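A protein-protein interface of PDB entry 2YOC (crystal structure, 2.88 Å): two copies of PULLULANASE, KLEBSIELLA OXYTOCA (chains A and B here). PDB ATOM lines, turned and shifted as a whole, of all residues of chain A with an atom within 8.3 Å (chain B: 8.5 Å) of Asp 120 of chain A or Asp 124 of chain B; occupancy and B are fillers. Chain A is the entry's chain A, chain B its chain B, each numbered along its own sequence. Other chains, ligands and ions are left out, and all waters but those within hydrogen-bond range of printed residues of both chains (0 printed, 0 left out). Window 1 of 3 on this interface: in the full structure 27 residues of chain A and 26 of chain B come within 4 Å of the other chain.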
ATOM      1  N   SER A  62      10.379 -19.024  14.043  1.00  0.00           N
ATOM      2  CA  SER A  62       9.276 -18.116  13.726  1.00  0.00           C
ATOM      3  C   SER A  62       8.266 -18.680  12.712  1.00  0.00           C
ATOM      4  O   SER A  62       7.098 -18.293  12.732  1.00  0.00           O
ATOM      5  CB  SER A  62       9.827 -16.772  13.259  1.00  0.00           C
ATOM      6  OG  SER A  62      10.746 -16.907  12.185  1.00  0.00           O
ATOM      7  N   LYS A  63       8.723 -19.621  11.855  1.00  0.00           N
ATOM      8  CA  LYS A  63       7.948 -20.303  10.812  1.00  0.00           C
ATOM      9  C   LYS A  63       7.025 -21.354  11.396  1.00  0.00           C
ATOM     10  O   LYS A  63       7.457 -22.178  12.206  1.00  0.00           O
ATOM     11  CB  LYS A  63       8.881 -20.912   9.739  1.00  0.00           C
ATOM     12  CG  LYS A  63       9.139 -20.010   8.520  1.00  0.00           C
ATOM     13  CD  LYS A  63       9.925 -18.747   8.834  1.00  0.00           C
ATOM     14  CE  LYS A  63      10.175 -17.921   7.615  1.00  0.00           C
ATOM     15  NZ  LYS A  63      11.129 -16.825   7.935  1.00  0.00           N
ATOM     16  N   ASN A  64       5.742 -21.302  11.001  1.00  0.00           N
ATOM     17  CA  ASN A  64       4.685 -22.206  11.470  1.00  0.00           C
ATOM     18  C   ASN A  64       3.515 -22.320  10.490  1.00  0.00           C
ATOM     19  O   ASN A  64       3.212 -21.376   9.758  1.00  0.00           O
ATOM     20  CB  ASN A  64       4.161 -21.769  12.848  1.00  0.00           C
ATOM     21  CG  ASN A  64       3.611 -20.356  12.898  1.00  0.00           C
ATOM     22  OD1 ASN A  64       4.304 -19.379  12.627  1.00  0.00           O
ATOM     23  ND2 ASN A  64       2.368 -20.212  13.304  1.00  0.00           N
ATOM     24  N   TRP A  83      -5.371 -19.916  16.620  1.00  0.00           N
ATOM     25  CA  TRP A  83      -4.722 -19.147  15.559  1.00  0.00           C
ATOM     26  C   TRP A  83      -3.433 -18.572  16.126  1.00  0.00           C
ATOM     27  O   TRP A  83      -2.444 -18.495  15.399  1.00  0.00           O
ATOM     28  CB  TRP A  83      -5.641 -18.032  15.015  1.00  0.00           C
ATOM     29  CG  TRP A  83      -4.953 -17.050  14.105  1.00  0.00           C
ATOM     30  CD1 TRP A  83      -4.408 -15.847  14.457  1.00  0.00           C
ATOM     31  CD2 TRP A  83      -4.673 -17.226  12.711  1.00  0.00           C
ATOM     32  NE1 TRP A  83      -3.827 -15.251  13.362  1.00  0.00           N
ATOM     33  CE2 TRP A  83      -3.965 -16.080  12.277  1.00  0.00           C
ATOM     34  CE3 TRP A  83      -4.974 -18.232  11.774  1.00  0.00           C
ATOM     35  CZ2 TRP A  83      -3.551 -15.917  10.948  1.00  0.00           C
ATOM     36  CZ3 TRP A  83      -4.562 -18.072  10.461  1.00  0.00           C
ATOM     37  CH2 TRP A  83      -3.863 -16.928  10.058  1.00  0.00           C
ATOM     38  N   VAL A  86       1.572 -20.812  17.521  1.00  0.00           N
ATOM     39  CA  VAL A  86       2.753 -20.778  16.665  1.00  0.00           C
ATOM     40  C   VAL A  86       3.563 -22.098  16.910  1.00  0.00           C
ATOM     41  O   VAL A  86       4.600 -22.306  16.283  1.00  0.00           O
ATOM     42  CB  VAL A  86       3.549 -19.454  16.953  1.00  0.00           C
ATOM     43  CG1 VAL A  86       4.871 -19.372  16.178  1.00  0.00           C
ATOM     44  CG2 VAL A  86       2.694 -18.221  16.659  1.00  0.00           C
ATOM     45  N   ILE A 114      -1.883 -22.868   5.824  1.00  0.00           N
ATOM     46  CA  ILE A 114      -1.618 -21.431   5.813  1.00  0.00           C
ATOM     47  C   ILE A 114      -0.200 -21.331   6.319  1.00  0.00           C
ATOM     48  O   ILE A 114       0.079 -21.640   7.483  1.00  0.00           O
ATOM     49  CB  ILE A 114      -2.618 -20.541   6.610  1.00  0.00           C
ATOM     50  CG1 ILE A 114      -4.027 -20.595   5.978  1.00  0.00           C
ATOM     51  CG2 ILE A 114      -2.096 -19.085   6.686  1.00  0.00           C
ATOM     52  CD1 ILE A 114      -5.151 -20.253   6.898  1.00  0.00           C
ATOM     53  N   VAL A 115       0.706 -20.992   5.413  1.00  0.00           N
ATOM     54  CA  VAL A 115       2.123 -20.876   5.708  1.00  0.00           C
ATOM     55  C   VAL A 115       2.380 -19.500   6.363  1.00  0.00           C
ATOM     56  O   VAL A 115       1.972 -18.474   5.817  1.00  0.00           O
ATOM     57  CB  VAL A 115       2.930 -21.143   4.423  1.00  0.00           C
ATOM     58  CG1 VAL A 115       4.399 -20.812   4.614  1.00  0.00           C
ATOM     59  CG2 VAL A 115       2.756 -22.590   3.958  1.00  0.00           C
ATOM     60  N   ARG A 116       2.986 -19.495   7.571  1.00  0.00           N
ATOM     61  CA  ARG A 116       3.217 -18.267   8.342  1.00  0.00           C
ATOM     62  C   ARG A 116       4.624 -18.125   8.957  1.00  0.00           C
ATOM     63  O   ARG A 116       5.352 -19.108   9.108  1.00  0.00           O
ATOM     64  CB  ARG A 116       2.195 -18.150   9.491  1.00  0.00           C
ATOM     65  CG  ARG A 116       0.723 -18.127   9.105  1.00  0.00           C
ATOM     66  CD  ARG A 116      -0.124 -17.843  10.331  1.00  0.00           C
ATOM     67  NE  ARG A 116      -0.256 -19.004  11.214  1.00  0.00           N
ATOM     68  CZ  ARG A 116      -0.535 -18.934  12.515  1.00  0.00           C
ATOM     69  NH1 ARG A 116      -0.673 -17.754  13.110  1.00  0.00           N
ATOM     70  NH2 ARG A 116      -0.654 -20.043  13.234  1.00  0.00           N
ATOM     71  N   ASP A 117       4.969 -16.873   9.335  1.00  0.00           N
ATOM     72  CA  ASP A 117       6.174 -16.434  10.047  1.00  0.00           C
ATOM     73  C   ASP A 117       5.592 -15.601  11.192  1.00  0.00           C
ATOM     74  O   ASP A 117       5.387 -14.385  11.076  1.00  0.00           O
ATOM     75  CB  ASP A 117       7.100 -15.588   9.136  1.00  0.00           C
ATOM     76  CG  ASP A 117       8.490 -15.261   9.694  1.00  0.00           C
ATOM     77  OD1 ASP A 117       8.625 -15.138  10.934  1.00  0.00           O
ATOM     78  OD2 ASP A 117       9.419 -15.034   8.880  1.00  0.00           O
ATOM     79  N   GLY A 118       5.245 -16.303  12.259  1.00  0.00           N
ATOM     80  CA  GLY A 118       4.549 -15.737  13.403  1.00  0.00           C
ATOM     81  C   GLY A 118       3.062 -15.841  13.136  1.00  0.00           C
ATOM     82  O   GLY A 118       2.586 -16.885  12.658  1.00  0.00           O
ATOM     83  N   THR A 119       2.323 -14.753  13.409  1.00  0.00           N
ATOM     84  CA  THR A 119       0.885 -14.748  13.150  1.00  0.00           C
ATOM     85  C   THR A 119       0.574 -13.942  11.881  1.00  0.00           C
ATOM     86  O   THR A 119      -0.436 -13.221  11.810  1.00  0.00           O
ATOM     87  CB  THR A 119       0.056 -14.531  14.441  1.00  0.00           C
ATOM     88  OG1 THR A 119      -1.261 -15.032  14.234  1.00  0.00           O
ATOM     89  CG2 THR A 119       0.031 -13.079  14.909  1.00  0.00           C
ATOM     90  N   ASP A 120       1.469 -14.088  10.870  1.00  0.00           N
ATOM     91  CA  ASP A 120       1.412 -13.405   9.575  1.00  0.00           C
ATOM     92  C   ASP A 120       1.542 -14.389   8.408  1.00  0.00           C
ATOM     93  O   ASP A 120       2.519 -15.138   8.346  1.00  0.00           O
ATOM     94  CB  ASP A 120       2.498 -12.314   9.482  1.00  0.00           C
ATOM     95  CG  ASP A 120       2.445 -11.208  10.526  1.00  0.00           C
ATOM     96  OD1 ASP A 120       1.335 -10.663  10.767  1.00  0.00           O
ATOM     97  OD2 ASP A 120       3.526 -10.831  11.049  1.00  0.00           O
ATOM     98  N   LYS A 121       0.552 -14.374   7.480  1.00  0.00           N
ATOM     99  CA  LYS A 121       0.503 -15.235   6.291  1.00  0.00           C
ATOM    100  C   LYS A 121       1.706 -14.986   5.388  1.00  0.00           C
ATOM    101  O   LYS A 121       1.948 -13.835   5.024  1.00  0.00           O
ATOM    102  CB  LYS A 121      -0.763 -14.947   5.466  1.00  0.00           C
ATOM    103  CG  LYS A 121      -2.064 -15.445   6.045  1.00  0.00           C
ATOM    104  CD  LYS A 121      -3.225 -15.038   5.118  1.00  0.00           C
ATOM    105  CE  LYS A 121      -3.972 -16.203   4.499  1.00  0.00           C
ATOM    106  NZ  LYS A 121      -3.155 -16.979   3.526  1.00  0.00           N
ATOM    107  N   LEU A 122       2.440 -16.051   5.018  1.00  0.00           N
ATOM    108  CA  LEU A 122       3.565 -15.951   4.089  1.00  0.00           C
ATOM    109  C   LEU A 122       3.051 -16.068   2.651  1.00  0.00           C
ATOM    110  O   LEU A 122       3.529 -15.361   1.764  1.00  0.00           O
ATOM    111  CB  LEU A 122       4.645 -17.000   4.381  1.00  0.00           C
ATOM    112  CG  LEU A 122       5.582 -16.696   5.548  1.00  0.00           C
ATOM    113  CD1 LEU A 122       6.375 -17.923   5.928  1.00  0.00           C
ATOM    114  CD2 LEU A 122       6.541 -15.539   5.229  1.00  0.00           C
ATOM    115  N   ILE A 123       2.067 -16.952   2.434  1.00  0.00           N
ATOM    116  CA  ILE A 123       1.402 -17.131   1.144  1.00  0.00           C
ATOM    117  C   ILE A 123       0.018 -16.485   1.263  1.00  0.00           C
ATOM    118  O   ILE A 123      -0.767 -16.879   2.132  1.00  0.00           O
ATOM    119  CB  ILE A 123       1.397 -18.611   0.652  1.00  0.00           C
ATOM    120  CG1 ILE A 123       2.761 -18.977   0.086  1.00  0.00           C
ATOM    121  CG2 ILE A 123       0.337 -18.863  -0.405  1.00  0.00           C
ATOM    122  CD1 ILE A 123       3.408 -20.067   0.794  1.00  0.00           C
ATOM    123  N   ASP A 124      -0.234 -15.451   0.416  1.00  0.00           N
ATOM    124  CA  ASP A 124      -1.462 -14.634   0.319  1.00  0.00           C
ATOM    125  C   ASP A 124      -2.764 -15.443   0.352  1.00  0.00           C
ATOM    126  O   ASP A 124      -3.627 -15.184   1.201  1.00  0.00           O
ATOM    127  CB  ASP A 124      -1.405 -13.672  -0.894  1.00  0.00           C
ATOM    128  CG  ASP A 124      -0.880 -14.281  -2.199  1.00  0.00           C
ATOM    129  OD1 ASP A 124       0.362 -14.292  -2.395  1.00  0.00           O
ATOM    130  OD2 ASP A 124      -1.714 -14.685  -3.052  1.00  0.00           O
ATOM    131  N   VAL B 113     -10.486 -10.487  17.442  1.00  0.00           N
ATOM    132  CA  VAL B 113     -10.972 -10.017  16.141  1.00  0.00           C
ATOM    133  C   VAL B 113      -9.831  -9.930  15.117  1.00  0.00           C
ATOM    134  O   VAL B 113      -8.786  -9.336  15.385  1.00  0.00           O
ATOM    135  CB  VAL B 113     -11.721  -8.658  16.229  1.00  0.00           C
ATOM    136  CG1 VAL B 113     -12.587  -8.423  14.992  1.00  0.00           C
ATOM    137  CG2 VAL B 113     -12.550  -8.549  17.502  1.00  0.00           C
ATOM    138  N   ILE B 114     -10.049 -10.521  13.940  1.00  0.00           N
ATOM    139  CA  ILE B 114      -9.133 -10.419  12.813  1.00  0.00           C
ATOM    140  C   ILE B 114      -9.979  -9.799  11.728  1.00  0.00           C
ATOM    141  O   ILE B 114     -10.928 -10.417  11.238  1.00  0.00           O
ATOM    142  CB  ILE B 114      -8.439 -11.740  12.377  1.00  0.00           C
ATOM    143  CG1 ILE B 114      -7.496 -12.264  13.486  1.00  0.00           C
ATOM    144  CG2 ILE B 114      -7.661 -11.519  11.070  1.00  0.00           C
ATOM    145  CD1 ILE B 114      -7.201 -13.743  13.443  1.00  0.00           C
ATOM    146  N   VAL B 115      -9.686  -8.544  11.427  1.00  0.00           N
ATOM    147  CA  VAL B 115     -10.400  -7.776  10.419  1.00  0.00           C
ATOM    148  C   VAL B 115      -9.849  -8.152   9.028  1.00  0.00           C
ATOM    149  O   VAL B 115      -8.637  -8.106   8.817  1.00  0.00           O
ATOM    150  CB  VAL B 115     -10.315  -6.267  10.764  1.00  0.00           C
ATOM    151  CG1 VAL B 115     -10.855  -5.399   9.631  1.00  0.00           C
ATOM    152  CG2 VAL B 115     -11.041  -5.967  12.076  1.00  0.00           C
ATOM    153  N   ASP B 120      -7.789 -12.379   3.725  1.00  0.00           N
ATOM    154  CA  ASP B 120      -6.604 -11.540   3.895  1.00  0.00           C
ATOM    155  C   ASP B 120      -6.790 -10.528   5.038  1.00  0.00           C
ATOM    156  O   ASP B 120      -7.750  -9.744   5.023  1.00  0.00           O
ATOM    157  CB  ASP B 120      -6.267 -10.802   2.574  1.00  0.00           C
ATOM    158  CG  ASP B 120      -5.962 -11.684   1.362  1.00  0.00           C
ATOM    159  OD1 ASP B 120      -5.187 -12.671   1.513  1.00  0.00           O
ATOM    160  OD2 ASP B 120      -6.430 -11.346   0.246  1.00  0.00           O
ATOM    161  N   LYS B 121      -5.848 -10.531   6.011  1.00  0.00           N
ATOM    162  CA  LYS B 121      -5.858  -9.649   7.181  1.00  0.00           C
ATOM    163  C   LYS B 121      -5.765  -8.185   6.768  1.00  0.00           C
ATOM    164  O   LYS B 121      -4.865  -7.819   6.011  1.00  0.00           O
ATOM    165  CB  LYS B 121      -4.664  -9.955   8.091  1.00  0.00           C
ATOM    166  CG  LYS B 121      -4.709 -11.260   8.858  1.00  0.00           C
ATOM    167  CD  LYS B 121      -3.407 -11.439   9.651  1.00  0.00           C
ATOM    168  CE  LYS B 121      -3.584 -11.447  11.151  1.00  0.00           C
ATOM    169  NZ  LYS B 121      -4.026 -10.129  11.695  1.00  0.00           N
ATOM    170  N   LEU B 122      -6.683  -7.347   7.265  1.00  0.00           N
ATOM    171  CA  LEU B 122      -6.659  -5.899   7.016  1.00  0.00           C
ATOM    172  C   LEU B 122      -5.786  -5.211   8.071  1.00  0.00           C
ATOM    173  O   LEU B 122      -5.045  -4.285   7.748  1.00  0.00           O
ATOM    174  CB  LEU B 122      -8.066  -5.294   6.997  1.00  0.00           C
ATOM    175  CG  LEU B 122      -8.875  -5.507   5.720  1.00  0.00           C
ATOM    176  CD1 LEU B 122     -10.316  -5.149   5.945  1.00  0.00           C
ATOM    177  CD2 LEU B 122      -8.340  -4.672   4.578  1.00  0.00           C
ATOM    178  N   ILE B 123      -5.855  -5.688   9.328  1.00  0.00           N
ATOM    179  CA  ILE B 123      -5.010  -5.221  10.428  1.00  0.00           C
ATOM    180  C   ILE B 123      -3.972  -6.318  10.692  1.00  0.00           C
ATOM    181  O   ILE B 123      -4.344  -7.463  10.976  1.00  0.00           O
ATOM    182  CB  ILE B 123      -5.828  -4.784  11.678  1.00  0.00           C
ATOM    183  CG1 ILE B 123      -6.438  -3.403  11.442  1.00  0.00           C
ATOM    184  CG2 ILE B 123      -4.977  -4.757  12.947  1.00  0.00           C
ATOM    185  CD1 ILE B 123      -7.886  -3.396  11.493  1.00  0.00           C
ATOM    186  N   ASP B 124      -2.676  -5.956  10.526  1.00  0.00           N
ATOM    187  CA  ASP B 124      -1.475  -6.799  10.677  1.00  0.00           C
ATOM    188  C   ASP B 124      -1.486  -7.683  11.942  1.00  0.00           C
ATOM    189  O   ASP B 124      -1.338  -8.908  11.839  1.00  0.00           O
ATOM    190  CB  ASP B 124      -0.175  -5.952  10.580  1.00  0.00           C
ATOM    191  CG  ASP B 124      -0.177  -4.622  11.327  1.00  0.00           C
ATOM    192  OD1 ASP B 124      -0.657  -3.615  10.751  1.00  0.00           O
ATOM    193  OD2 ASP B 124       0.340  -4.579  12.473  1.00  0.00           O
ATOM    194  N   SER B 125      -1.700  -7.055  13.113  1.00  0.00           N
ATOM    195  CA  SER B 125      -1.769  -7.701  14.420  1.00  0.00           C
ATOM    196  C   SER B 125      -3.168  -8.268  14.709  1.00  0.00           C
ATOM    197  O   SER B 125      -4.182  -7.734  14.229  1.00  0.00           O
ATOM    198  CB  SER B 125      -1.363  -6.719  15.522  1.00  0.00           C
ATOM    199  OG  SER B 125      -2.236  -5.603  15.634  1.00  0.00           O
ATOM    200  N   ASP B 126      -3.213  -9.362  15.502  1.00  0.00           N
ATOM    201  CA  ASP B 126      -4.459  -9.972  15.956  1.00  0.00           C
ATOM    202  C   ASP B 126      -4.991  -9.051  17.061  1.00  0.00           C
ATOM    203  O   ASP B 126      -4.309  -8.834  18.072  1.00  0.00           O
ATOM    204  CB  ASP B 126      -4.219 -11.390  16.511  1.00  0.00           C
ATOM    205  CG  ASP B 126      -3.545 -12.379  15.582  1.00  0.00           C
ATOM    206  OD1 ASP B 126      -3.373 -12.055  14.387  1.00  0.00           O
ATOM    207  OD2 ASP B 126      -3.193 -13.482  16.051  1.00  0.00           O
ATOM    208  N   LEU B 127      -6.166  -8.456  16.839  1.00  0.00           N
ATOM    209  CA  LEU B 127      -6.755  -7.547  17.813  1.00  0.00           C
ATOM    210  C   LEU B 127      -7.300  -8.306  19.014  1.00  0.00           C
ATOM    211  O   LEU B 127      -7.781  -9.437  18.878  1.00  0.00           O
ATOM    212  CB  LEU B 127      -7.877  -6.704  17.188  1.00  0.00           C
ATOM    213  CG  LEU B 127      -7.538  -5.878  15.952  1.00  0.00           C
ATOM    214  CD1 LEU B 127      -8.808  -5.498  15.191  1.00  0.00           C
ATOM    215  CD2 LEU B 127      -6.729  -4.639  16.317  1.00  0.00           C
ATOM    216  N   ILE B 142      -8.878   1.102  11.977  1.00  0.00           N
ATOM    217  CA  ILE B 142      -8.505   1.519  10.612  1.00  0.00           C
ATOM    218  C   ILE B 142      -7.590   0.431  10.037  1.00  0.00           C
ATOM    219  O   ILE B 142      -6.815  -0.153  10.792  1.00  0.00           O
ATOM    220  CB  ILE B 142      -7.799   2.907  10.559  1.00  0.00           C
ATOM    221  CG1 ILE B 142      -8.390   3.925  11.551  1.00  0.00           C
ATOM    222  CG2 ILE B 142      -7.788   3.466   9.131  1.00  0.00           C
ATOM    223  CD1 ILE B 142      -7.349   4.931  12.065  1.00  0.00           C
ATOM    224  N   ALA B 143      -7.666   0.162   8.718  1.00  0.00           N
ATOM    225  CA  ALA B 143      -6.839  -0.864   8.071  1.00  0.00           C
ATOM    226  C   ALA B 143      -5.328  -0.619   8.194  1.00  0.00           C
ATOM    227  O   ALA B 143      -4.854   0.483   7.906  1.00  0.00           O
ATOM    228  CB  ALA B 143      -7.238  -1.032   6.615  1.00  0.00           C
ATOM    229  N   GLY B 144      -4.617  -1.650   8.672  1.00  0.00           N
ATOM    230  CA  GLY B 144      -3.170  -1.662   8.903  1.00  0.00           C
ATOM    231  C   GLY B 144      -2.691  -0.823  10.079  1.00  0.00           C
ATOM    232  O   GLY B 144      -1.486  -0.610  10.233  1.00  0.00           O
ATOM    233  N   ASN B 145      -3.636  -0.366  10.929  1.00  0.00           N
ATOM    234  CA  ASN B 145      -3.409   0.525  12.068  1.00  0.00           C
ATOM    235  C   ASN B 145      -3.039  -0.163  13.375  1.00  0.00           C
ATOM    236  O   ASN B 145      -2.375   0.475  14.196  1.00  0.00           O
ATOM    237  CB  ASN B 145      -4.612   1.453  12.267  1.00  0.00           C
ATOM    238  CG  ASN B 145      -4.339   2.715  13.046  1.00  0.00           C
ATOM    239  OD1 ASN B 145      -4.577   2.782  14.248  1.00  0.00           O
ATOM    240  ND2 ASN B 145      -3.892   3.764  12.367  1.00  0.00           N
ATOM    241  N   SER B 146      -3.477  -1.439  13.594  1.00  0.00           N
ATOM    242  CA  SER B 146      -3.234  -2.248  14.816  1.00  0.00           C
ATOM    243  C   SER B 146      -3.889  -1.691  16.084  1.00  0.00           C
ATOM    244  O   SER B 146      -4.120  -2.449  17.033  1.00  0.00           O
ATOM    245  CB  SER B 146      -1.742  -2.477  15.062  1.00  0.00           C
ATOM    246  OG  SER B 146      -1.182  -3.420  14.163  1.00  0.00           O
ATOM    247  N   ALA B 147      -4.163  -0.371  16.107  1.00  0.00           N
ATOM    248  CA  ALA B 147      -4.740   0.341  17.241  1.00  0.00           C
ATOM    249  C   ALA B 147      -6.254   0.291  17.257  1.00  0.00           C
ATOM    250  O   ALA B 147      -6.902   0.209  16.210  1.00  0.00           O
ATOM    251  CB  ALA B 147      -4.261   1.783  17.257  1.00  0.00           C
ATOM    252  N   LEU B 164       3.554   6.988  11.483  1.00  0.00           N
ATOM    253  CA  LEU B 164       4.907   6.454  11.192  1.00  0.00           C
ATOM    254  C   LEU B 164       6.035   7.524  11.234  1.00  0.00           C
ATOM    255  O   LEU B 164       5.774   8.664  11.616  1.00  0.00           O
ATOM    256  CB  LEU B 164       4.943   5.635   9.867  1.00  0.00           C
ATOM    257  CG  LEU B 164       3.767   4.686   9.572  1.00  0.00           C
ATOM    258  CD1 LEU B 164       3.574   4.504   8.091  1.00  0.00           C
ATOM    259  CD2 LEU B 164       3.951   3.356  10.230  1.00  0.00           C
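The guanidinium group (NH1) of Arg 116 of chain A lies within hydrogen-bond range of the backbone carbonyl oxygen (O) of Trp 83 of chain A, at 3.0 Å.
The guanidinium group (NH1) of Arg 116 of chain A lies within hydrogen-bond range of the side-chain hydroxyl (OG1) of Thr 119 of chain A (3.0 Å).
O of Asp 124 of chain A sits at hydrogen-bond distance from NZ of Lys 121 of chain A, at 3.0 Å.
O of Asp 124 of chain B lies within hydrogen-bond range of NZ of Lys 121 of chain B (3.0 Å).
The side-chain amino group of Lys 121 of chain B lies within hydrogen-bond range of the backbone carbonyl oxygen of Ser 125 of chain B (3.5 Å).
The side-chain carboxylate of Asp 124 of chain B is in hydrogen-bond range of the side-chain hydroxyl of Ser 146 of chain B (2.6 Å).
Asp 120 of chain A touches Asp 124 of chain B, and with the chains exchanged Asp 124 of chain A touches Asp 120 of chain B.
7 positions are printed for both chains.
Of the 6 pairs that touch across the chains among the printed residues, 2 have their exchanged pair printed and touching as well.
CD1 of Trp 83 of chain A touches CD1 of Ile 114 of chain B, 3.6 Å away.
Thr 119 of chain A touches Lys 121 of chain B.
Of the 18 printed residues of chain B, 5 touch a printed residue of chain A.
Hydrophobic or aromatic side chains of chain B that line the printed part of chain A: Ile 114.
Hydrophobic or aromatic side chains of chain A that line the printed part of chain B: Trp 83.
Among the printed residues, 6 pairs touch across the chains.
Among the printed residues, no Asp or Glu carboxylate lies within 4 Å of a Lys or Arg side-chain nitrogen of the other chain.
Val 86 of chain A touches none of the printed residues of chain B.
Of chain B, only Lys 121 (3.7 Å) and Asp 126 (3.1 Å) come within 4 Å of Thr 119 of chain A.
Asp 120 of chain A touches just one residue of chain B: Asp 124.
Printed residues of chain B within 4 Å of Asp 124 of chain A: Asp 120.
Of the printed residues of chain A, Ile 114 of chain B touches Trp 83.
Printed residues of chain A within 4 Å of Asp 124 of chain B: Asp 120 (3.4 Å).
Ala 147 of chain B touches none of the printed residues of chain A.
The nearest residue of chain B that does not touch Asp 120 of chain A is Lys 121 of chain B (4.9 Å).
The nearest residue of chain A that does not touch Asp 124 of chain B is Thr 119 of chain A (4.4 Å).
The side-chain carboxylate (OD2) of Asp 126 of chain B lies close to the indole nitrogen (NE1) of Trp 83 of chain A.
The side-chain hydroxyl (OG1) of Thr 119 of chain A lies within hydrogen-bond range of the side-chain carboxylate (OD2) of Asp 126 of chain B (3.1 Å).
OD1 of Asp 120 of chain A lies close to O of Asp 124 of chain B, at 3.4 Å.
The backbone carbonyl oxygen of Asp 124 of chain A sits close to the side-chain carboxylate of Asp 120 of chain B (3.0 Å).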
